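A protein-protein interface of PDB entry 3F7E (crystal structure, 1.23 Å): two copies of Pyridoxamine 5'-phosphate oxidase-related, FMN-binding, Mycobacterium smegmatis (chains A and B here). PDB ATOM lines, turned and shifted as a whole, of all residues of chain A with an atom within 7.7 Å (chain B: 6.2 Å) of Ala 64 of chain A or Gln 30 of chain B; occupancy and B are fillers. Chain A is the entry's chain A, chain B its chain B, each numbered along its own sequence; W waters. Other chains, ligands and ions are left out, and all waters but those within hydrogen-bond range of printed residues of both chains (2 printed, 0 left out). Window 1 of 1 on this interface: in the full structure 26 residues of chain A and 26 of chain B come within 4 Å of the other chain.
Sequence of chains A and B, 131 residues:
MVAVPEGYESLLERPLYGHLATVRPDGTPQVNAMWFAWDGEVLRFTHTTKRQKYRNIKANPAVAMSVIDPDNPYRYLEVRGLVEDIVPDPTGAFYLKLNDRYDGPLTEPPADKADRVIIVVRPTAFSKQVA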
ATOM      1  N   GLY A  18     -10.713  31.002  27.382  1.00  0.00           N
ATOM      2  CA  GLY A  18     -11.258  29.860  26.685  1.00  0.00           C
ATOM      3  C   GLY A  18     -10.814  28.571  27.358  1.00  0.00           C
ATOM      4  O   GLY A  18      -9.645  28.414  27.680  1.00  0.00           O
ATOM      5  N   HIS A  19     -11.739  27.646  27.538  1.00  0.00           N
ATOM      6  CA  HIS A  19     -11.427  26.404  28.254  1.00  0.00           C
ATOM      7  C   HIS A  19     -11.197  25.372  27.158  1.00  0.00           C
ATOM      8  O   HIS A  19     -12.112  24.938  26.471  1.00  0.00           O
ATOM      9  CB  HIS A  19     -12.567  26.064  29.212  1.00  0.00           C
ATOM     10  CG  HIS A  19     -12.666  27.052  30.323  1.00  0.00           C
ATOM     11  ND1 HIS A  19     -13.169  28.342  30.241  1.00  0.00           N
ATOM     12  CD2 HIS A  19     -12.251  26.886  31.600  1.00  0.00           C
ATOM     13  CE1 HIS A  19     -13.061  28.907  31.444  1.00  0.00           C
ATOM     14  NE2 HIS A  19     -12.509  28.040  32.274  1.00  0.00           N
ATOM     15  N   LEU A  20      -9.923  25.021  26.960  1.00  0.00           N
ATOM     16  CA  LEU A  20      -9.459  24.218  25.817  1.00  0.00           C
ATOM     17  C   LEU A  20      -9.307  22.768  26.229  1.00  0.00           C
ATOM     18  O   LEU A  20      -8.543  22.459  27.142  1.00  0.00           O
ATOM     19  CB  LEU A  20      -8.114  24.772  25.283  1.00  0.00           C
ATOM     20  CG  LEU A  20      -7.598  24.023  24.054  1.00  0.00           C
ATOM     21  CD1 LEU A  20      -8.498  24.291  22.817  1.00  0.00           C
ATOM     22  CD2 LEU A  20      -6.172  24.459  23.754  1.00  0.00           C
ATOM     23  N   ALA A  21     -10.058  21.906  25.542  1.00  0.00           N
ATOM     24  CA  ALA A  21     -10.053  20.463  25.801  1.00  0.00           C
ATOM     25  C   ALA A  21      -9.253  19.727  24.753  1.00  0.00           C
ATOM     26  O   ALA A  21      -9.368  19.997  23.536  1.00  0.00           O
ATOM     27  CB  ALA A  21     -11.484  19.924  25.803  1.00  0.00           C
ATOM     28  N   THR A  22      -8.475  18.770  25.215  1.00  0.00           N
ATOM     29  CA  THR A  22      -7.680  17.886  24.387  1.00  0.00           C
ATOM     30  C   THR A  22      -7.957  16.457  24.881  1.00  0.00           C
ATOM     31  O   THR A  22      -8.584  16.264  25.903  1.00  0.00           O
ATOM     32  CB  THR A  22      -6.176  18.218  24.495  1.00  0.00           C
ATOM     33  OG1 THR A  22      -5.754  18.183  25.870  1.00  0.00           O
ATOM     34  CG2 THR A  22      -5.832  19.569  23.841  1.00  0.00           C
ATOM     35  N   VAL A  23      -7.475  15.458  24.147  1.00  0.00           N
ATOM     36  CA  VAL A  23      -7.679  14.073  24.557  1.00  0.00           C
ATOM     37  C   VAL A  23      -6.310  13.438  24.720  1.00  0.00           C
ATOM     38  O   VAL A  23      -5.438  13.592  23.851  1.00  0.00           O
ATOM     39  CB  VAL A  23      -8.546  13.267  23.532  1.00  0.00           C
ATOM     40  CG1 VAL A  23      -8.906  11.923  24.086  1.00  0.00           C
ATOM     41  CG2 VAL A  23      -9.815  13.996  23.192  1.00  0.00           C
ATOM     42  N   PRO A  29     -10.180  12.781  28.581  1.00  0.00           N
ATOM     43  CA  PRO A  29     -10.008  14.206  28.253  1.00  0.00           C
ATOM     44  C   PRO A  29      -9.219  14.994  29.283  1.00  0.00           C
ATOM     45  O   PRO A  29      -9.087  14.591  30.449  1.00  0.00           O
ATOM     46  CB  PRO A  29     -11.450  14.703  28.153  1.00  0.00           C
ATOM     47  CG  PRO A  29     -12.193  13.861  29.169  1.00  0.00           C
ATOM     48  CD  PRO A  29     -11.518  12.507  29.171  1.00  0.00           C
ATOM     49  N   GLN A  30      -8.718  16.132  28.823  1.00  0.00           N
ATOM     50  CA  GLN A  30      -8.024  17.133  29.627  1.00  0.00           C
ATOM     51  C   GLN A  30      -8.641  18.482  29.235  1.00  0.00           C
ATOM     52  O   GLN A  30      -8.905  18.699  28.053  1.00  0.00           O
ATOM     53  CB  GLN A  30      -6.517  17.146  29.256  1.00  0.00           C
ATOM     54  CG  GLN A  30      -5.765  18.162  30.047  1.00  0.00           C
ATOM     55  CD  GLN A  30      -4.283  18.032  29.944  1.00  0.00           C
ATOM     56  OE1 GLN A  30      -3.588  19.038  30.055  1.00  0.00           O
ATOM     57  NE2 GLN A  30      -3.775  16.811  29.750  1.00  0.00           N
ATOM     58  N   VAL A  31      -8.834  19.405  30.191  1.00  0.00           N
ATOM     59  CA  VAL A  31      -9.337  20.733  29.843  1.00  0.00           C
ATOM     60  C   VAL A  31      -8.682  21.759  30.769  1.00  0.00           C
ATOM     61  O   VAL A  31      -8.554  21.552  31.993  1.00  0.00           O
ATOM     62  CB  VAL A  31     -10.896  20.776  29.863  1.00  0.00           C
ATOM     63  CG1 VAL A  31     -11.457  20.434  31.232  1.00  0.00           C
ATOM     64  CG2 VAL A  31     -11.417  22.115  29.413  1.00  0.00           C
ATOM     65  N   ASN A  32      -8.292  22.885  30.195  1.00  0.00           N
ATOM     66  CA  ASN A  32      -7.556  23.919  30.922  1.00  0.00           C
ATOM     67  C   ASN A  32      -8.016  25.297  30.481  1.00  0.00           C
ATOM     68  O   ASN A  32      -8.228  25.542  29.286  1.00  0.00           O
ATOM     69  CB  ASN A  32      -6.050  23.821  30.643  1.00  0.00           C
ATOM     70  CG  ASN A  32      -5.491  22.483  31.027  1.00  0.00           C
ATOM     71  OD1 ASN A  32      -5.315  22.210  32.226  1.00  0.00           O
ATOM     72  ND2 ASN A  32      -5.248  21.610  30.036  1.00  0.00           N
ATOM     73  N   LEU A  43      -7.636  30.207  15.774  1.00  0.00           N
ATOM     74  CA  LEU A  43      -7.323  30.466  17.193  1.00  0.00           C
ATOM     75  C   LEU A  43      -5.855  30.149  17.430  1.00  0.00           C
ATOM     76  O   LEU A  43      -5.330  29.173  16.877  1.00  0.00           O
ATOM     77  CB  LEU A  43      -8.158  29.537  18.092  1.00  0.00           C
ATOM     78  CG  LEU A  43      -9.668  29.831  18.095  1.00  0.00           C
ATOM     79  CD1 LEU A  43     -10.470  28.605  18.581  1.00  0.00           C
ATOM     80  CD2 LEU A  43      -9.994  31.084  18.928  1.00  0.00           C
ATOM     81  N   PHE A  45      -2.864  29.717  20.659  1.00  0.00           N
ATOM     82  CA  PHE A  45      -2.601  29.518  22.088  1.00  0.00           C
ATOM     83  C   PHE A  45      -1.102  29.456  22.336  1.00  0.00           C
ATOM     84  O   PHE A  45      -0.348  29.080  21.448  1.00  0.00           O
ATOM     85  CB  PHE A  45      -3.211  28.188  22.566  1.00  0.00           C
ATOM     86  CG  PHE A  45      -4.675  28.045  22.246  1.00  0.00           C
ATOM     87  CD1 PHE A  45      -5.111  27.540  20.999  1.00  0.00           C
ATOM     88  CD2 PHE A  45      -5.629  28.432  23.177  1.00  0.00           C
ATOM     89  CE1 PHE A  45      -6.464  27.422  20.720  1.00  0.00           C
ATOM     90  CE2 PHE A  45      -6.971  28.315  22.905  1.00  0.00           C
ATOM     91  CZ  PHE A  45      -7.397  27.819  21.673  1.00  0.00           C
ATOM     92  N   PRO A  61      -4.787  15.651  17.060  1.00  0.00           N
ATOM     93  CA  PRO A  61      -4.881  17.105  16.828  1.00  0.00           C
ATOM     94  C   PRO A  61      -6.269  17.707  17.076  1.00  0.00           C
ATOM     95  O   PRO A  61      -6.433  18.924  16.930  1.00  0.00           O
ATOM     96  CB  PRO A  61      -4.465  17.248  15.358  1.00  0.00           C
ATOM     97  CG  PRO A  61      -4.918  15.983  14.756  1.00  0.00           C
ATOM     98  CD  PRO A  61      -4.670  14.916  15.789  1.00  0.00           C
ATOM     99  N   ALA A  62      -7.260  16.897  17.428  1.00  0.00           N
ATOM    100  CA  ALA A  62      -8.612  17.415  17.604  1.00  0.00           C
ATOM    101  C   ALA A  62      -8.774  18.055  18.975  1.00  0.00           C
ATOM    102  O   ALA A  62      -8.450  17.446  20.002  1.00  0.00           O
ATOM    103  CB  ALA A  62      -9.643  16.329  17.393  1.00  0.00           C
ATOM    104  N   VAL A  63      -9.319  19.263  18.996  1.00  0.00           N
ATOM    105  CA  VAL A  63      -9.498  20.023  20.215  1.00  0.00           C
ATOM    106  C   VAL A  63     -10.905  20.641  20.254  1.00  0.00           C
ATOM    107  O   VAL A  63     -11.632  20.660  19.247  1.00  0.00           O
ATOM    108  CB  VAL A  63      -8.434  21.141  20.366  1.00  0.00           C
ATOM    109  CG1 VAL A  63      -7.051  20.545  20.335  1.00  0.00           C
ATOM    110  CG2 VAL A  63      -8.600  22.267  19.317  1.00  0.00           C
ATOM    111  N   ALA A  64     -11.277  21.178  21.413  1.00  0.00           N
ATOM    112  CA  ALA A  64     -12.534  21.913  21.543  1.00  0.00           C
ATOM    113  C   ALA A  64     -12.320  23.027  22.558  1.00  0.00           C
ATOM    114  O   ALA A  64     -11.605  22.836  23.522  1.00  0.00           O
ATOM    115  CB  ALA A  64     -13.673  20.984  21.984  1.00  0.00           C
ATOM    116  N   MET A  65     -12.956  24.181  22.358  1.00  0.00           N
ATOM    117  CA  MET A  65     -12.808  25.314  23.296  1.00  0.00           C
ATOM    118  C   MET A  65     -14.182  25.861  23.633  1.00  0.00           C
ATOM    119  O   MET A  65     -15.038  26.070  22.761  1.00  0.00           O
ATOM    120  CB  MET A  65     -11.969  26.448  22.680  1.00  0.00           C
ATOM    121  CG  MET A  65     -11.615  27.529  23.681  1.00  0.00           C
ATOM    122  SD  MET A  65     -10.660  29.033  22.917  1.00  0.00           S
ATOM    123  CE  MET A  65     -12.180  29.967  22.157  1.00  0.00           C
ATOM    124  N   SER A  66     -14.391  26.097  24.922  1.00  0.00           N
ATOM    125  CA  SER A  66     -15.618  26.679  25.471  1.00  0.00           C
ATOM    126  C   SER A  66     -15.321  28.064  26.032  1.00  0.00           C
ATOM    127  O   SER A  66     -14.436  28.250  26.879  1.00  0.00           O
ATOM    128  CB  SER A  66     -16.136  25.759  26.594  1.00  0.00           C
ATOM    129  OG  SER A  66     -17.155  26.406  27.345  1.00  0.00           O
ATOM    130  N   GLU A  78     -19.085  27.414  21.726  1.00  0.00           N
ATOM    131  CA  GLU A  78     -18.270  26.198  21.747  1.00  0.00           C
ATOM    132  C   GLU A  78     -17.657  26.011  20.373  1.00  0.00           C
ATOM    133  O   GLU A  78     -18.385  25.959  19.377  1.00  0.00           O
ATOM    134  CB  GLU A  78     -19.144  24.981  22.096  1.00  0.00           C
ATOM    135  CG  GLU A  78     -19.812  25.093  23.453  1.00  0.00           C
ATOM    136  CD  GLU A  78     -20.961  24.152  23.626  1.00  0.00           C
ATOM    137  OE1 GLU A  78     -21.148  23.284  22.750  1.00  0.00           O
ATOM    138  OE2 GLU A  78     -21.695  24.265  24.644  1.00  0.00           O
ATOM    139  N   VAL A  79     -16.325  25.910  20.316  1.00  0.00           N
ATOM    140  CA  VAL A  79     -15.594  25.791  19.048  1.00  0.00           C
ATOM    141  C   VAL A  79     -14.864  24.457  18.988  1.00  0.00           C
ATOM    142  O   VAL A  79     -13.973  24.237  19.772  1.00  0.00           O
ATOM    143  CB  VAL A  79     -14.524  26.910  18.896  1.00  0.00           C
ATOM    144  CG1 VAL A  79     -13.868  26.882  17.490  1.00  0.00           C
ATOM    145  CG2 VAL A  79     -15.125  28.317  19.175  1.00  0.00           C
ATOM    146  N   ARG A  80     -15.199  23.577  18.056  1.00  0.00           N
ATOM    147  CA  ARG A  80     -14.376  22.364  17.841  1.00  0.00           C
ATOM    148  C   ARG A  80     -13.423  22.656  16.686  1.00  0.00           C
ATOM    149  O   ARG A  80     -13.743  23.473  15.811  1.00  0.00           O
ATOM    150  CB  ARG A  80     -15.260  21.154  17.568  1.00  0.00           C
ATOM    151  CG  ARG A  80     -16.053  20.718  18.804  1.00  0.00           C
ATOM    152  CD  ARG A  80     -17.361  20.042  18.428  1.00  0.00           C
ATOM    153  NE  ARG A  80     -17.109  18.896  17.573  1.00  0.00           N
ATOM    154  CZ  ARG A  80     -17.946  18.476  16.621  1.00  0.00           C
ATOM    155  NH1 ARG A  80     -17.599  17.432  15.872  1.00  0.00           N
ATOM    156  NH2 ARG A  80     -19.122  19.102  16.392  1.00  0.00           N
ATOM    157  N   GLY A  81     -12.252  22.037  16.677  1.00  0.00           N
ATOM    158  CA  GLY A  81     -11.322  22.327  15.585  1.00  0.00           C
ATOM    159  C   GLY A  81     -10.152  21.372  15.603  1.00  0.00           C
ATOM    160  O   GLY A  81     -10.111  20.411  16.389  1.00  0.00           O
ATOM    161  N   LEU A  82      -9.214  21.635  14.701  1.00  0.00           N
ATOM    162  CA  LEU A  82      -8.015  20.824  14.557  1.00  0.00           C
ATOM    163  C   LEU A  82      -6.774  21.685  14.665  1.00  0.00           C
ATOM    164  O   LEU A  82      -6.707  22.790  14.070  1.00  0.00           O
ATOM    165  CB  LEU A  82      -8.017  20.133  13.185  1.00  0.00           C
ATOM    166  CG  LEU A  82      -9.094  19.063  12.951  1.00  0.00           C
ATOM    167  CD1 LEU A  82      -9.179  18.673  11.493  1.00  0.00           C
ATOM    168  CD2 LEU A  82      -8.865  17.825  13.804  1.00  0.00           C
ATOM    169  N   VAL A 121      -5.105  26.595  15.703  1.00  0.00           N
ATOM    170  CA  VAL A 121      -6.280  25.737  15.584  1.00  0.00           C
ATOM    171  C   VAL A 121      -7.266  26.331  14.575  1.00  0.00           C
ATOM    172  O   VAL A 121      -7.661  27.498  14.681  1.00  0.00           O
ATOM    173  CB  VAL A 121      -6.998  25.607  16.953  1.00  0.00           C
ATOM    174  CG1 VAL A 121      -8.370  24.939  16.821  1.00  0.00           C
ATOM    175  CG2 VAL A 121      -6.106  24.866  17.944  1.00  0.00           C
ATOM    176  N   ALA A 125     -16.254  23.374  13.727  1.00  0.00           N
ATOM    177  CA  ALA A 125     -17.662  23.460  14.124  1.00  0.00           C
ATOM    178  C   ALA A 125     -17.825  24.516  15.217  1.00  0.00           C
ATOM    179  O   ALA A 125     -16.916  24.744  16.019  1.00  0.00           O
ATOM    180  CB  ALA A 125     -18.195  22.097  14.628  1.00  0.00           C
ATOM    181  N   LEU B  20     -17.069  21.416  31.253  1.00  0.00           N
ATOM    182  CA  LEU B  20     -16.990  19.955  31.355  1.00  0.00           C
ATOM    183  C   LEU B  20     -16.626  19.392  29.985  1.00  0.00           C
ATOM    184  O   LEU B  20     -17.348  19.587  29.015  1.00  0.00           O
ATOM    185  CB  LEU B  20     -18.325  19.376  31.828  1.00  0.00           C
ATOM    186  CG  LEU B  20     -18.315  17.848  32.075  1.00  0.00           C
ATOM    187  CD1 LEU B  20     -17.366  17.497  33.242  1.00  0.00           C
ATOM    188  CD2 LEU B  20     -19.702  17.318  32.394  1.00  0.00           C
ATOM    189  N   ALA B  21     -15.504  18.690  29.939  1.00  0.00           N
ATOM    190  CA  ALA B  21     -14.995  18.022  28.750  1.00  0.00           C
ATOM    191  C   ALA B  21     -15.346  16.540  28.768  1.00  0.00           C
ATOM    192  O   ALA B  21     -15.173  15.841  29.783  1.00  0.00           O
ATOM    193  CB  ALA B  21     -13.494  18.203  28.660  1.00  0.00           C
ATOM    194  N   THR B  22     -15.859  16.097  27.616  1.00  0.00           N
ATOM    195  CA  THR B  22     -16.198  14.700  27.362  1.00  0.00           C
ATOM    196  C   THR B  22     -15.532  14.295  26.045  1.00  0.00           C
ATOM    197  O   THR B  22     -15.007  15.160  25.295  1.00  0.00           O
ATOM    198  CB  THR B  22     -17.729  14.473  27.301  1.00  0.00           C
ATOM    199  OG1 THR B  22     -18.306  15.332  26.300  1.00  0.00           O
ATOM    200  CG2 THR B  22     -18.383  14.781  28.647  1.00  0.00           C
ATOM    201  N   VAL B  23     -15.553  12.987  25.760  1.00  0.00           N
ATOM    202  CA  VAL B  23     -15.010  12.496  24.500  1.00  0.00           C
ATOM    203  C   VAL B  23     -16.143  11.946  23.665  1.00  0.00           C
ATOM    204  O   VAL B  23     -16.966  11.145  24.149  1.00  0.00           O
ATOM    205  CB  VAL B  23     -13.911  11.417  24.740  1.00  0.00           C
ATOM    206  CG1 VAL B  23     -13.233  11.066  23.445  1.00  0.00           C
ATOM    207  CG2 VAL B  23     -12.844  11.947  25.704  1.00  0.00           C
ATOM    208  N   ARG B  24     -16.183  12.379  22.402  1.00  0.00           N
ATOM    209  CA  ARG B  24     -17.233  11.967  21.485  1.00  0.00           C
ATOM    210  C   ARG B  24     -16.957  10.559  20.956  1.00  0.00           C
ATOM    211  O   ARG B  24     -15.833  10.055  21.045  1.00  0.00           O
ATOM    212  CB  ARG B  24     -17.297  12.951  20.304  1.00  0.00           C
ATOM    213  CG  ARG B  24     -17.702  14.362  20.755  1.00  0.00           C
ATOM    214  CD  ARG B  24     -17.456  15.423  19.686  1.00  0.00           C
ATOM    215  NE  ARG B  24     -18.341  15.288  18.531  1.00  0.00           N
ATOM    216  CZ  ARG B  24     -19.501  15.942  18.366  1.00  0.00           C
ATOM    217  NH1 ARG B  24     -19.979  16.746  19.307  1.00  0.00           N
ATOM    218  NH2 ARG B  24     -20.182  15.809  17.240  1.00  0.00           N
ATOM    219  N   THR B  28     -12.846  12.483  19.471  1.00  0.00           N
ATOM    220  CA  THR B  28     -12.471  13.886  19.580  1.00  0.00           C
ATOM    221  C   THR B  28     -13.181  14.505  20.795  1.00  0.00           C
ATOM    222  O   THR B  28     -14.215  14.017  21.229  1.00  0.00           O
ATOM    223  CB  THR B  28     -12.825  14.700  18.288  1.00  0.00           C
ATOM    224  OG1 THR B  28     -14.244  14.809  18.177  1.00  0.00           O
ATOM    225  CG2 THR B  28     -12.243  14.065  17.017  1.00  0.00           C
ATOM    226  N   PRO B  29     -12.605  15.575  21.367  1.00  0.00           N
ATOM    227  CA  PRO B  29     -13.200  16.140  22.594  1.00  0.00           C
ATOM    228  C   PRO B  29     -14.353  17.101  22.327  1.00  0.00           C
ATOM    229  O   PRO B  29     -14.498  17.673  21.230  1.00  0.00           O
ATOM    230  CB  PRO B  29     -12.029  16.894  23.224  1.00  0.00           C
ATOM    231  CG  PRO B  29     -11.225  17.344  22.034  1.00  0.00           C
ATOM    232  CD  PRO B  29     -11.343  16.254  21.009  1.00  0.00           C
ATOM    233  N   GLN B  30     -15.134  17.328  23.375  1.00  0.00           N
ATOM    234  CA  GLN B  30     -16.182  18.291  23.395  1.00  0.00           C
ATOM    235  C   GLN B  30     -16.109  18.964  24.765  1.00  0.00           C
ATOM    236  O   GLN B  30     -15.793  18.309  25.742  1.00  0.00           O
ATOM    237  CB  GLN B  30     -17.503  17.528  23.270  1.00  0.00           C
ATOM    238  CG  GLN B  30     -18.695  18.400  23.285  1.00  0.00           C
ATOM    239  CD  GLN B  30     -19.993  17.638  23.086  1.00  0.00           C
ATOM    240  OE1 GLN B  30     -20.999  17.937  23.766  1.00  0.00           O
ATOM    241  NE2 GLN B  30     -20.010  16.679  22.160  1.00  0.00           N
ATOM    242  N   VAL B  31     -16.490  20.242  24.844  1.00  0.00           N
ATOM    243  CA  VAL B  31     -16.506  20.951  26.127  1.00  0.00           C
ATOM    244  C   VAL B  31     -17.708  21.897  26.181  1.00  0.00           C
ATOM    245  O   VAL B  31     -17.981  22.630  25.226  1.00  0.00           O
ATOM    246  CB  VAL B  31     -15.144  21.631  26.441  1.00  0.00           C
ATOM    247  CG1 VAL B  31     -14.668  22.552  25.338  1.00  0.00           C
ATOM    248  CG2 VAL B  31     -15.181  22.334  27.786  1.00  0.00           C
ATOM    249  N   ASN B  32     -18.433  21.844  27.308  1.00  0.00           N
ATOM    250  CA  ASN B  32     -19.675  22.594  27.525  1.00  0.00           C
ATOM    251  C   ASN B  32     -19.663  23.253  28.892  1.00  0.00           C
ATOM    252  O   ASN B  32     -19.303  22.618  29.874  1.00  0.00           O
ATOM    253  CB  ASN B  32     -20.879  21.648  27.465  1.00  0.00           C
ATOM    254  CG  ASN B  32     -20.986  20.934  26.128  1.00  0.00           C
ATOM    255  OD1 ASN B  32     -21.522  21.493  25.151  1.00  0.00           O
ATOM    256  ND2 ASN B  32     -20.529  19.713  26.071  1.00  0.00           N
ATOM    257  N   GLN B  52     -25.966  15.439  22.976  1.00  0.00           N
ATOM    258  CA  GLN B  52     -24.719  14.740  22.653  1.00  0.00           C
ATOM    259  C   GLN B  52     -23.843  14.469  23.879  1.00  0.00           C
ATOM    260  O   GLN B  52     -23.243  13.391  23.969  1.00  0.00           O
ATOM    261  CB  GLN B  52     -23.927  15.490  21.576  1.00  0.00           C
ATOM    262  CG  GLN B  52     -22.725  14.714  21.046  1.00  0.00           C
ATOM    263  CD  GLN B  52     -23.153  13.410  20.375  1.00  0.00           C
ATOM    264  OE1 GLN B  52     -24.054  13.419  19.545  1.00  0.00           O
ATOM    265  NE2 GLN B  52     -22.544  12.281  20.748  1.00  0.00           N
ATOM    266  N   LYS B  53     -23.753  15.417  24.816  1.00  0.00           N
ATOM    267  CA  LYS B  53     -22.850  15.221  25.941  1.00  0.00           C
ATOM    268  C   LYS B  53     -23.287  13.999  26.767  1.00  0.00           C
ATOM    269  O   LYS B  53     -22.435  13.267  27.295  1.00  0.00           O
ATOM    270  CB  LYS B  53     -22.712  16.492  26.804  1.00  0.00           C
ATOM    271  CG  LYS B  53     -23.990  17.095  27.338  1.00  0.00           C
ATOM    272  CD  LYS B  53     -23.745  18.508  27.913  1.00  0.00           C
ATOM    273  CE  LYS B  53     -24.947  19.428  27.656  1.00  0.00           C
ATOM    274  NZ  LYS B  53     -24.913  20.675  28.488  1.00  0.00           N
ATOM    275  N   ASN B  56     -22.162  10.975  24.873  1.00  0.00           N
ATOM    276  CA  ASN B  56     -20.720  10.820  25.018  1.00  0.00           C
ATOM    277  C   ASN B  56     -20.397  10.019  26.284  1.00  0.00           C
ATOM    278  O   ASN B  56     -19.590   9.077  26.263  1.00  0.00           O
ATOM    279  CB  ASN B  56     -20.009  12.179  25.111  1.00  0.00           C
ATOM    280  CG  ASN B  56     -20.082  12.981  23.837  1.00  0.00           C
ATOM    281  OD1 ASN B  56     -20.462  12.467  22.764  1.00  0.00           O
ATOM    282  ND2 ASN B  56     -19.679  14.235  23.929  1.00  0.00           N
HETATM  283  O   HOH W   1     -15.208  15.932  15.266  1.00  0.00           O
HETATM  284  O   HOH W   2     -14.826  17.479  18.511  1.00  0.00           O
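The backbone carbonyl oxygen (O) of Thr 22 of chain B lies within hydrogen-bond range of the backbone NH (N) of Gln 30 of chain B, 2.9 Å away. The backbone carbonyl oxygen (O) of Ala 64 of chain A sits at hydrogen-bond distance from the backbone NH (N) of Ala 21 of chain A (2.7 Å). The backbone carbonyl oxygen (O) of Met 65 of chain A is in hydrogen-bond range of the backbone NH (N) of Val 79 of chain A (2.8 Å). NH1 of Arg 24 of chain B sits close to NE2 of Gln 30 of chain B (2.9 Å). N of Leu 20 of chain B sits at hydrogen-bond distance from O of Asn 32 of chain B (2.9 Å). N of His 19 of chain A is in hydrogen-bond range of O of Ser 66 of chain A, 2.8 Å away.
Ala 21 of chain B touches its own counterpart, Ala 21 of chain A. Ala 21 of chain A touches Pro 29 of chain B, and with the chains exchanged Pro 29 of chain A touches Ala 21 of chain B. Val 23 of chain A touches Pro 29 of chain B, and with the chains exchanged Pro 29 of chain A touches Val 23 of chain B. Val 31 of chain A touches Ala 21 of chain B, but with the chains exchanged Ala 21 of chain A does not touch Val 31 of chain B (4.1 Å). Of the 18 pairs that touch across the chains among the printed residues, 5 have their exchanged pair printed and touching as well.
Printed residues of chain A that touch a printed residue of chain B: His 19, Ala 21, Val 23, Pro 29, Val 31, Ala 62, Val 63, Ala 64, Met 65, Ser 66, Glu 78 and Arg 80. Of the 13 printed residues of chain B, 8 touch a printed residue of chain A. Printed residues of chain B that touch a printed residue of chain A: Ala 21, Val 23, Arg 24, Thr 28, Pro 29, Gln 30, Val 31 and Asn 32. Among the printed residues, 18 pairs touch across the chains.
Val 31 of chain B touches His 19 of chain A. CG2 of Val 23 of chain A touches CD of Pro 29 of chain B (3.5 Å). CD of Pro 29 of chain A touches CG2 of Val 23 of chain B, 3.8 Å away. Ala 21 of chain B touches Val 31 of chain A (CB to CB, 3.8 Å). Ala 62 of chain A touches Thr 28 of chain B. Ala 62 of chain A touches Pro 29 of chain B (O to CD, 3.3 Å). CB of Ala 64 of chain A touches O of Pro 29 of chain B (3.5 Å). O of Ala 64 of chain A touches CG1 of Val 31 of chain B, at 3.6 Å. Val 31 of chain B touches Ser 66 of chain A (CG1 to N, 3.6 Å). Val 31 of chain B touches Glu 78 of chain A.
Ala 64 of chain A touches just these residues of chain B: Pro 29, Gln 30 and Val 31. Of the printed residues of chain A, Pro 29 of chain B touches Ala 21, Val 23, Ala 62, Val 63 and Ala 64. Printed residues of chain B within 4 Å of Glu 78 of chain A: Val 31 and Asn 32. Printed residues of chain B within 4 Å of Met 65 of chain A: Val 31 (3.8 Å). Of the printed residues of chain B, Ala 21 of chain A touches Ala 21 (3.9 Å) and Pro 29 (3.6 Å). Pro 61 of chain A touches none of the printed residues of chain B.
The guanidinium group (NH1) of Arg 80 of chain A lies close to the guanidinium group (NH2) of Arg 24 of chain B (3.3 Å). The side-chain carboxylate (OE2) of Glu 78 of chain A sits close to the side-chain amide oxygen (OD1) of Asn 32 of chain B, at 2.8 Å.
Water W2 lies within hydrogen-bond range of O of Pro 29 of chain B (2.7 Å), OG1 of Thr 28 of chain B (2.8 Å) and NE of Arg 80 of chain A (2.8 Å). Water W1 lies within hydrogen-bond range of the guanidinium group of Arg 80 of chain A (2.9 Å) and the side-chain hydroxyl of Thr 28 of chain B (3.3 Å).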
